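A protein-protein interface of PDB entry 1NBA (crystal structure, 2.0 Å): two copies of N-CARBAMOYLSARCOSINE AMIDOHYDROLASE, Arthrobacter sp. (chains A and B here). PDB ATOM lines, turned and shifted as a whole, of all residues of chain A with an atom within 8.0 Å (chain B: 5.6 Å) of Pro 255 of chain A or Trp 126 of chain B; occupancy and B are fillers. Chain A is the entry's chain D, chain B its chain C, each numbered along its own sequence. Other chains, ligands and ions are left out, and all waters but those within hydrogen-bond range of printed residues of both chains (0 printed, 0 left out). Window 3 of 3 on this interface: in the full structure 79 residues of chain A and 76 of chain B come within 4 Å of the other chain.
The side-chain carboxylate of Asp 257 of chain A sits at hydrogen-bond distance from the backbone NH of Tyr 125 of chain B, at 3.0 Å. NE1 of Trp 126 of chain B sits at hydrogen-bond distance from O of Pro 255 of chain A (3.0 Å).
No position is printed for both chains. Of the 11 pairs that touch across the chains among the printed residues, none has its exchanged pair printed and touching as well.
The side-chain amide oxygen (OD1) of Asn 54 of chain B lies close to the backbone carbonyl oxygen (O) of Tyr 125 of chain B, 3.2 Å away. N of Ala 55 of chain B sits at hydrogen-bond distance from O of Trp 126 of chain B (3.1 Å). NE2 of His 61 of chain B is in hydrogen-bond range of O of Thr 119 of chain B. The side-chain hydroxyl (OG) of Ser 124 of chain B is in hydrogen-bond range of the backbone carbonyl oxygen (O) of Pro 121 of chain B (3.0 Å). N of Trp 126 of chain B lies close to OG of Ser 124 of chain B (3.2 Å). The side-chain hydroxyl (OG) of Ser 124 of chain B sits at hydrogen-bond distance from the backbone NH (N) of Ala 127 of chain B, at 3.0 Å.
Trp 126 of chain B touches just these residues of chain A: Pro 255 (3.0 Å), Ala 256 (3.5 Å) and Asp 257 (3.5 Å). Printed residues of chain B within 4 Å of Val 252 of chain A: Thr 119 (3.5 Å). Of the printed residues of chain B, Asp 257 of chain A touches Ser 124, Tyr 125 and Trp 126. Of the printed residues of chain B, Ala 254 of chain A touches Thr 119. Of the printed residues of chain B, Pro 258 of chain A touches Tyr 125. Gly 60 of chain B touches none of the printed residues of chain A. Thr 93 of chain B touches none of the printed residues of chain A. The nearest printed residue of chain B that does not touch Asp 257 of chain A is Pro 121 of chain B (5.8 Å).
O of Val 252 of chain A touches CG2 of Thr 119 of chain B, at 3.5 Å. Glu 253 of chain A touches Thr 119 of chain B (O to CG2, 3.6 Å). Thr 119 of chain B touches Ala 254 of chain A. NE2 of His 61 of chain B touches CD of Pro 255 of chain A, 3.5 Å away. Pro 62 of chain B touches Pro 255 of chain A. Ala 256 of chain A touches Trp 126 of chain B. Asp 257 of chain A touches Ser 124 of chain B (OD1 to CB, 3.6 Å). Asp 257 of chain A touches Trp 126 of chain B (OD1 to CD1, 3.5 Å). Pro 258 of chain A touches Tyr 125 of chain B.
Printed residues of chain A that touch a printed residue of chain B: Val 252, Glu 253, Ala 254, Pro 255, Ala 256, Asp 257 and Pro 258. Among the printed residues, 11 pairs touch across the chains. Among the printed residues, no Asp or Glu carboxylate lies within 4 Å of a Lys or Arg side-chain nitrogen of the other chain.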
ATOM      1  N   VAL A 252      -3.392   3.151  25.421  1.00  0.00           N
ATOM      2  CA  VAL A 252      -2.564   3.675  26.485  1.00  0.00           C
ATOM      3  C   VAL A 252      -2.724   5.192  26.340  1.00  0.00           C
ATOM      4  O   VAL A 252      -2.845   5.740  25.235  1.00  0.00           O
ATOM      5  CB  VAL A 252      -1.094   3.241  26.260  1.00  0.00           C
ATOM      6  CG1 VAL A 252      -0.207   3.785  27.376  1.00  0.00           C
ATOM      7  CG2 VAL A 252      -0.992   1.720  26.262  1.00  0.00           C
ATOM      8  N   GLU A 253      -2.733   5.881  27.474  1.00  0.00           N
ATOM      9  CA  GLU A 253      -2.915   7.318  27.519  1.00  0.00           C
ATOM     10  C   GLU A 253      -1.596   8.034  27.259  1.00  0.00           C
ATOM     11  O   GLU A 253      -0.534   7.555  27.663  1.00  0.00           O
ATOM     12  CB  GLU A 253      -3.486   7.651  28.898  1.00  0.00           C
ATOM     13  CG  GLU A 253      -4.033   9.058  29.106  1.00  0.00           C
ATOM     14  CD  GLU A 253      -4.610   9.279  30.505  1.00  0.00           C
ATOM     15  N   ALA A 254      -1.627   9.147  26.526  1.00  0.00           N
ATOM     16  CA  ALA A 254      -0.432   9.946  26.306  1.00  0.00           C
ATOM     17  C   ALA A 254       0.056  10.496  27.650  1.00  0.00           C
ATOM     18  O   ALA A 254      -0.777  10.903  28.469  1.00  0.00           O
ATOM     19  CB  ALA A 254      -0.742  11.117  25.381  1.00  0.00           C
ATOM     20  N   PRO A 255       1.358  10.454  27.964  1.00  0.00           N
ATOM     21  CA  PRO A 255       1.940  11.150  29.104  1.00  0.00           C
ATOM     22  C   PRO A 255       1.708  12.650  29.024  1.00  0.00           C
ATOM     23  O   PRO A 255       1.870  13.271  27.969  1.00  0.00           O
ATOM     24  CB  PRO A 255       3.406  10.776  29.068  1.00  0.00           C
ATOM     25  CG  PRO A 255       3.341   9.397  28.484  1.00  0.00           C
ATOM     26  CD  PRO A 255       2.335   9.566  27.357  1.00  0.00           C
ATOM     27  N   ALA A 256       1.302  13.220  30.152  1.00  0.00           N
ATOM     28  CA  ALA A 256       1.079  14.654  30.253  1.00  0.00           C
ATOM     29  C   ALA A 256       2.383  15.419  30.082  1.00  0.00           C
ATOM     30  O   ALA A 256       3.456  14.937  30.451  1.00  0.00           O
ATOM     31  CB  ALA A 256       0.512  15.015  31.613  1.00  0.00           C
ATOM     32  N   ASP A 257       2.283  16.596  29.477  1.00  0.00           N
ATOM     33  CA  ASP A 257       3.435  17.453  29.270  1.00  0.00           C
ATOM     34  C   ASP A 257       3.779  18.124  30.584  1.00  0.00           C
ATOM     35  O   ASP A 257       2.859  18.480  31.318  1.00  0.00           O
ATOM     36  CB  ASP A 257       3.123  18.524  28.249  1.00  0.00           C
ATOM     37  CG  ASP A 257       3.076  18.100  26.790  1.00  0.00           C
ATOM     38  OD1 ASP A 257       3.025  16.909  26.466  1.00  0.00           O
ATOM     39  OD2 ASP A 257       3.098  19.010  25.968  1.00  0.00           O
ATOM     40  N   PRO A 258       5.050  18.318  30.942  1.00  0.00           N
ATOM     41  CA  PRO A 258       5.455  19.216  32.018  1.00  0.00           C
ATOM     42  C   PRO A 258       5.066  20.685  31.815  1.00  0.00           C
ATOM     43  O   PRO A 258       4.822  21.436  32.764  1.00  0.00           O
ATOM     44  CB  PRO A 258       6.954  18.983  32.120  1.00  0.00           C
ATOM     45  CG  PRO A 258       7.337  18.412  30.780  1.00  0.00           C
ATOM     46  CD  PRO A 258       6.165  17.486  30.510  1.00  0.00           C
ATOM     47  N   ALA B  53      14.026  12.325  20.381  1.00  0.00           N
ATOM     48  CA  ALA B  53      13.077  13.321  20.826  1.00  0.00           C
ATOM     49  C   ALA B  53      12.720  12.899  22.231  1.00  0.00           C
ATOM     50  O   ALA B  53      12.954  11.746  22.626  1.00  0.00           O
ATOM     51  CB  ALA B  53      11.806  13.324  19.983  1.00  0.00           C
ATOM     52  N   ASN B  54      12.122  13.785  23.020  1.00  0.00           N
ATOM     53  CA  ASN B  54      11.906  13.546  24.440  1.00  0.00           C
ATOM     54  C   ASN B  54      11.183  12.295  24.828  1.00  0.00           C
ATOM     55  O   ASN B  54      11.514  11.711  25.854  1.00  0.00           O
ATOM     56  CB  ASN B  54      11.195  14.743  25.061  1.00  0.00           C
ATOM     57  CG  ASN B  54      12.098  15.970  25.111  1.00  0.00           C
ATOM     58  OD1 ASN B  54      11.653  17.106  25.004  1.00  0.00           O
ATOM     59  ND2 ASN B  54      13.410  15.834  25.284  1.00  0.00           N
ATOM     60  N   ALA B  55      10.264  11.800  24.005  1.00  0.00           N
ATOM     61  CA  ALA B  55       9.593  10.531  24.284  1.00  0.00           C
ATOM     62  C   ALA B  55      10.529   9.324  24.372  1.00  0.00           C
ATOM     63  O   ALA B  55      10.210   8.324  25.015  1.00  0.00           O
ATOM     64  CB  ALA B  55       8.571  10.237  23.191  1.00  0.00           C
ATOM     65  N   TRP B  56      11.643   9.390  23.641  1.00  0.00           N
ATOM     66  CA  TRP B  56      12.621   8.318  23.614  1.00  0.00           C
ATOM     67  C   TRP B  56      13.763   8.657  24.571  1.00  0.00           C
ATOM     68  O   TRP B  56      14.202   7.791  25.326  1.00  0.00           O
ATOM     69  CB  TRP B  56      13.166   8.124  22.168  1.00  0.00           C
ATOM     70  CG  TRP B  56      12.100   7.617  21.187  1.00  0.00           C
ATOM     71  CD1 TRP B  56      11.928   6.276  20.997  1.00  0.00           C
ATOM     72  CD2 TRP B  56      11.187   8.375  20.475  1.00  0.00           C
ATOM     73  NE1 TRP B  56      10.911   6.178  20.177  1.00  0.00           N
ATOM     74  CE2 TRP B  56      10.441   7.387  19.845  1.00  0.00           C
ATOM     75  CE3 TRP B  56      10.874   9.709  20.257  1.00  0.00           C
ATOM     76  CZ2 TRP B  56       9.374   7.703  19.013  1.00  0.00           C
ATOM     77  CZ3 TRP B  56       9.814  10.031  19.425  1.00  0.00           C
ATOM     78  CH2 TRP B  56       9.070   9.036  18.809  1.00  0.00           C
ATOM     79  N   GLN B  58      13.894  10.941  27.191  1.00  0.00           N
ATOM     80  CA  GLN B  58      13.537  11.285  28.542  1.00  0.00           C
ATOM     81  C   GLN B  58      12.807  10.088  29.077  1.00  0.00           C
ATOM     82  O   GLN B  58      12.165   9.367  28.320  1.00  0.00           O
ATOM     83  CB  GLN B  58      12.657  12.524  28.550  1.00  0.00           C
ATOM     84  CG  GLN B  58      13.388  13.750  28.008  1.00  0.00           C
ATOM     85  CD  GLN B  58      14.619  14.090  28.818  1.00  0.00           C
ATOM     86  OE1 GLN B  58      14.566  14.081  30.040  1.00  0.00           O
ATOM     87  NE2 GLN B  58      15.794  14.310  28.238  1.00  0.00           N
ATOM     88  N   PRO B  59      12.963   9.766  30.359  1.00  0.00           N
ATOM     89  CA  PRO B  59      12.205   8.714  31.018  1.00  0.00           C
ATOM     90  C   PRO B  59      10.728   9.041  31.165  1.00  0.00           C
ATOM     91  O   PRO B  59      10.305  10.198  31.073  1.00  0.00           O
ATOM     92  CB  PRO B  59      12.906   8.545  32.344  1.00  0.00           C
ATOM     93  CG  PRO B  59      13.372   9.955  32.635  1.00  0.00           C
ATOM     94  CD  PRO B  59      13.907  10.391  31.282  1.00  0.00           C
ATOM     95  N   GLY B  60       9.928   8.018  31.406  1.00  0.00           N
ATOM     96  CA  GLY B  60       8.525   8.239  31.662  1.00  0.00           C
ATOM     97  C   GLY B  60       7.607   8.069  30.462  1.00  0.00           C
ATOM     98  O   GLY B  60       6.395   8.009  30.675  1.00  0.00           O
ATOM     99  N   HIS B  61       8.038   7.991  29.210  1.00  0.00           N
ATOM    100  CA  HIS B  61       7.084   7.776  28.133  1.00  0.00           C
ATOM    101  C   HIS B  61       7.059   6.271  27.831  1.00  0.00           C
ATOM    102  O   HIS B  61       8.086   5.615  28.002  1.00  0.00           O
ATOM    103  CB  HIS B  61       7.536   8.586  26.926  1.00  0.00           C
ATOM    104  CG  HIS B  61       6.431   8.766  25.894  1.00  0.00           C
ATOM    105  ND1 HIS B  61       5.976   7.889  25.001  1.00  0.00           N
ATOM    106  CD2 HIS B  61       5.678   9.919  25.762  1.00  0.00           C
ATOM    107  CE1 HIS B  61       4.987   8.465  24.356  1.00  0.00           C
ATOM    108  NE2 HIS B  61       4.814   9.671  24.820  1.00  0.00           N
ATOM    109  N   PRO B  62       6.008   5.614  27.304  1.00  0.00           N
ATOM    110  CA  PRO B  62       6.098   4.229  26.821  1.00  0.00           C
ATOM    111  C   PRO B  62       7.165   3.981  25.752  1.00  0.00           C
ATOM    112  O   PRO B  62       7.585   2.860  25.497  1.00  0.00           O
ATOM    113  CB  PRO B  62       4.686   3.918  26.360  1.00  0.00           C
ATOM    114  CG  PRO B  62       3.998   5.247  26.252  1.00  0.00           C
ATOM    115  CD  PRO B  62       4.612   6.022  27.398  1.00  0.00           C
ATOM    116  N   THR B  93      11.109  12.930  14.164  1.00  0.00           N
ATOM    117  CA  THR B  93      10.375  12.720  15.396  1.00  0.00           C
ATOM    118  C   THR B  93       9.151  11.944  14.895  1.00  0.00           C
ATOM    119  O   THR B  93       8.677  12.145  13.770  1.00  0.00           O
ATOM    120  CB  THR B  93      10.023  14.086  16.081  1.00  0.00           C
ATOM    121  OG1 THR B  93       9.292  13.686  17.235  1.00  0.00           O
ATOM    122  CG2 THR B  93       9.230  15.082  15.268  1.00  0.00           C
ATOM    123  N   VAL B  95       5.500  11.427  15.268  1.00  0.00           N
ATOM    124  CA  VAL B  95       4.344  11.973  15.972  1.00  0.00           C
ATOM    125  C   VAL B  95       3.086  12.047  15.119  1.00  0.00           C
ATOM    126  O   VAL B  95       3.164  12.074  13.886  1.00  0.00           O
ATOM    127  CB  VAL B  95       4.660  13.400  16.522  1.00  0.00           C
ATOM    128  CG1 VAL B  95       5.489  13.236  17.799  1.00  0.00           C
ATOM    129  CG2 VAL B  95       5.387  14.256  15.482  1.00  0.00           C
ATOM    130  N   THR B 119       0.156   7.442  21.966  1.00  0.00           N
ATOM    131  CA  THR B 119       0.833   8.180  23.021  1.00  0.00           C
ATOM    132  C   THR B 119       1.802   9.226  22.478  1.00  0.00           C
ATOM    133  O   THR B 119       2.531   9.881  23.247  1.00  0.00           O
ATOM    134  CB  THR B 119       1.562   7.167  23.964  1.00  0.00           C
ATOM    135  OG1 THR B 119       2.619   6.543  23.231  1.00  0.00           O
ATOM    136  CG2 THR B 119       0.598   6.137  24.538  1.00  0.00           C
ATOM    137  N   PRO B 121       1.690  12.571  20.536  1.00  0.00           N
ATOM    138  CA  PRO B 121       1.128  13.779  19.960  1.00  0.00           C
ATOM    139  C   PRO B 121       2.127  14.682  19.256  1.00  0.00           C
ATOM    140  O   PRO B 121       3.247  14.903  19.747  1.00  0.00           O
ATOM    141  CB  PRO B 121       0.472  14.488  21.128  1.00  0.00           C
ATOM    142  CG  PRO B 121       0.592  13.577  22.331  1.00  0.00           C
ATOM    143  CD  PRO B 121       1.813  12.745  21.985  1.00  0.00           C
ATOM    144  N   SER B 124       3.728  18.257  21.159  1.00  0.00           N
ATOM    145  CA  SER B 124       3.775  18.029  22.584  1.00  0.00           C
ATOM    146  C   SER B 124       5.237  18.211  22.967  1.00  0.00           C
ATOM    147  O   SER B 124       6.122  18.219  22.098  1.00  0.00           O
ATOM    148  CB  SER B 124       3.339  16.604  22.909  1.00  0.00           C
ATOM    149  OG  SER B 124       4.284  15.667  22.414  1.00  0.00           O
ATOM    150  N   TYR B 125       5.476  18.244  24.280  1.00  0.00           N
ATOM    151  CA  TYR B 125       6.823  18.294  24.827  1.00  0.00           C
ATOM    152  C   TYR B 125       7.557  17.051  24.325  1.00  0.00           C
ATOM    153  O   TYR B 125       8.689  17.090  23.857  1.00  0.00           O
ATOM    154  CB  TYR B 125       6.749  18.294  26.362  1.00  0.00           C
ATOM    155  CG  TYR B 125       8.094  18.040  27.040  1.00  0.00           C
ATOM    156  CD1 TYR B 125       9.033  19.049  27.109  1.00  0.00           C
ATOM    157  CD2 TYR B 125       8.370  16.781  27.543  1.00  0.00           C
ATOM    158  CE1 TYR B 125      10.261  18.794  27.676  1.00  0.00           C
ATOM    159  CE2 TYR B 125       9.593  16.526  28.112  1.00  0.00           C
ATOM    160  CZ  TYR B 125      10.528  17.535  28.167  1.00  0.00           C
ATOM    161  OH  TYR B 125      11.770  17.276  28.713  1.00  0.00           O
ATOM    162  N   TRP B 126       6.818  15.943  24.351  1.00  0.00           N
ATOM    163  CA  TRP B 126       7.355  14.662  23.957  1.00  0.00           C
ATOM    164  C   TRP B 126       7.794  14.578  22.510  1.00  0.00           C
ATOM    165  O   TRP B 126       8.666  13.771  22.174  1.00  0.00           O
ATOM    166  CB  TRP B 126       6.323  13.609  24.250  1.00  0.00           C
ATOM    167  CG  TRP B 126       6.002  13.563  25.738  1.00  0.00           C
ATOM    168  CD1 TRP B 126       4.732  13.834  26.175  1.00  0.00           C
ATOM    169  CD2 TRP B 126       6.866  13.229  26.758  1.00  0.00           C
ATOM    170  NE1 TRP B 126       4.787  13.656  27.467  1.00  0.00           N
ATOM    171  CE2 TRP B 126       6.026  13.296  27.855  1.00  0.00           C
ATOM    172  CE3 TRP B 126       8.195  12.876  26.916  1.00  0.00           C
ATOM    173  CZ2 TRP B 126       6.500  13.014  29.121  1.00  0.00           C
ATOM    174  CZ3 TRP B 126       8.670  12.592  28.182  1.00  0.00           C
ATOM    175  CH2 TRP B 126       7.830  12.661  29.275  1.00  0.00           C
ATOM    176  N   ALA B 127       7.225  15.414  21.655  1.00  0.00           N
ATOM    177  CA  ALA B 127       7.598  15.448  20.258  1.00  0.00           C
ATOM    178  C   ALA B 127       8.890  16.210  20.048  1.00  0.00           C
ATOM    179  O   ALA B 127       9.452  16.128  18.950  1.00  0.00           O
ATOM    180  CB  ALA B 127       6.530  16.144  19.436  1.00  0.00           C
ATOM    181  N   GLN B 128       9.393  16.996  21.000  1.00  0.00           N
ATOM    182  CA  GLN B 128      10.581  17.802  20.768  1.00  0.00           C
ATOM    183  C   GLN B 128      11.898  17.075  20.752  1.00  0.00           C
ATOM    184  O   GLN B 128      12.102  16.123  21.504  1.00  0.00           O
ATOM    185  CB  GLN B 128      10.753  18.883  21.800  1.00  0.00           C
ATOM    186  CG  GLN B 128      10.307  20.224  21.277  1.00  0.00           C
ATOM    187  CD  GLN B 128       8.846  20.453  21.552  1.00  0.00           C
ATOM    188  OE1 GLN B 128       8.515  20.900  22.650  1.00  0.00           O
ATOM    189  NE2 GLN B 128       7.950  20.178  20.607  1.00  0.00           N
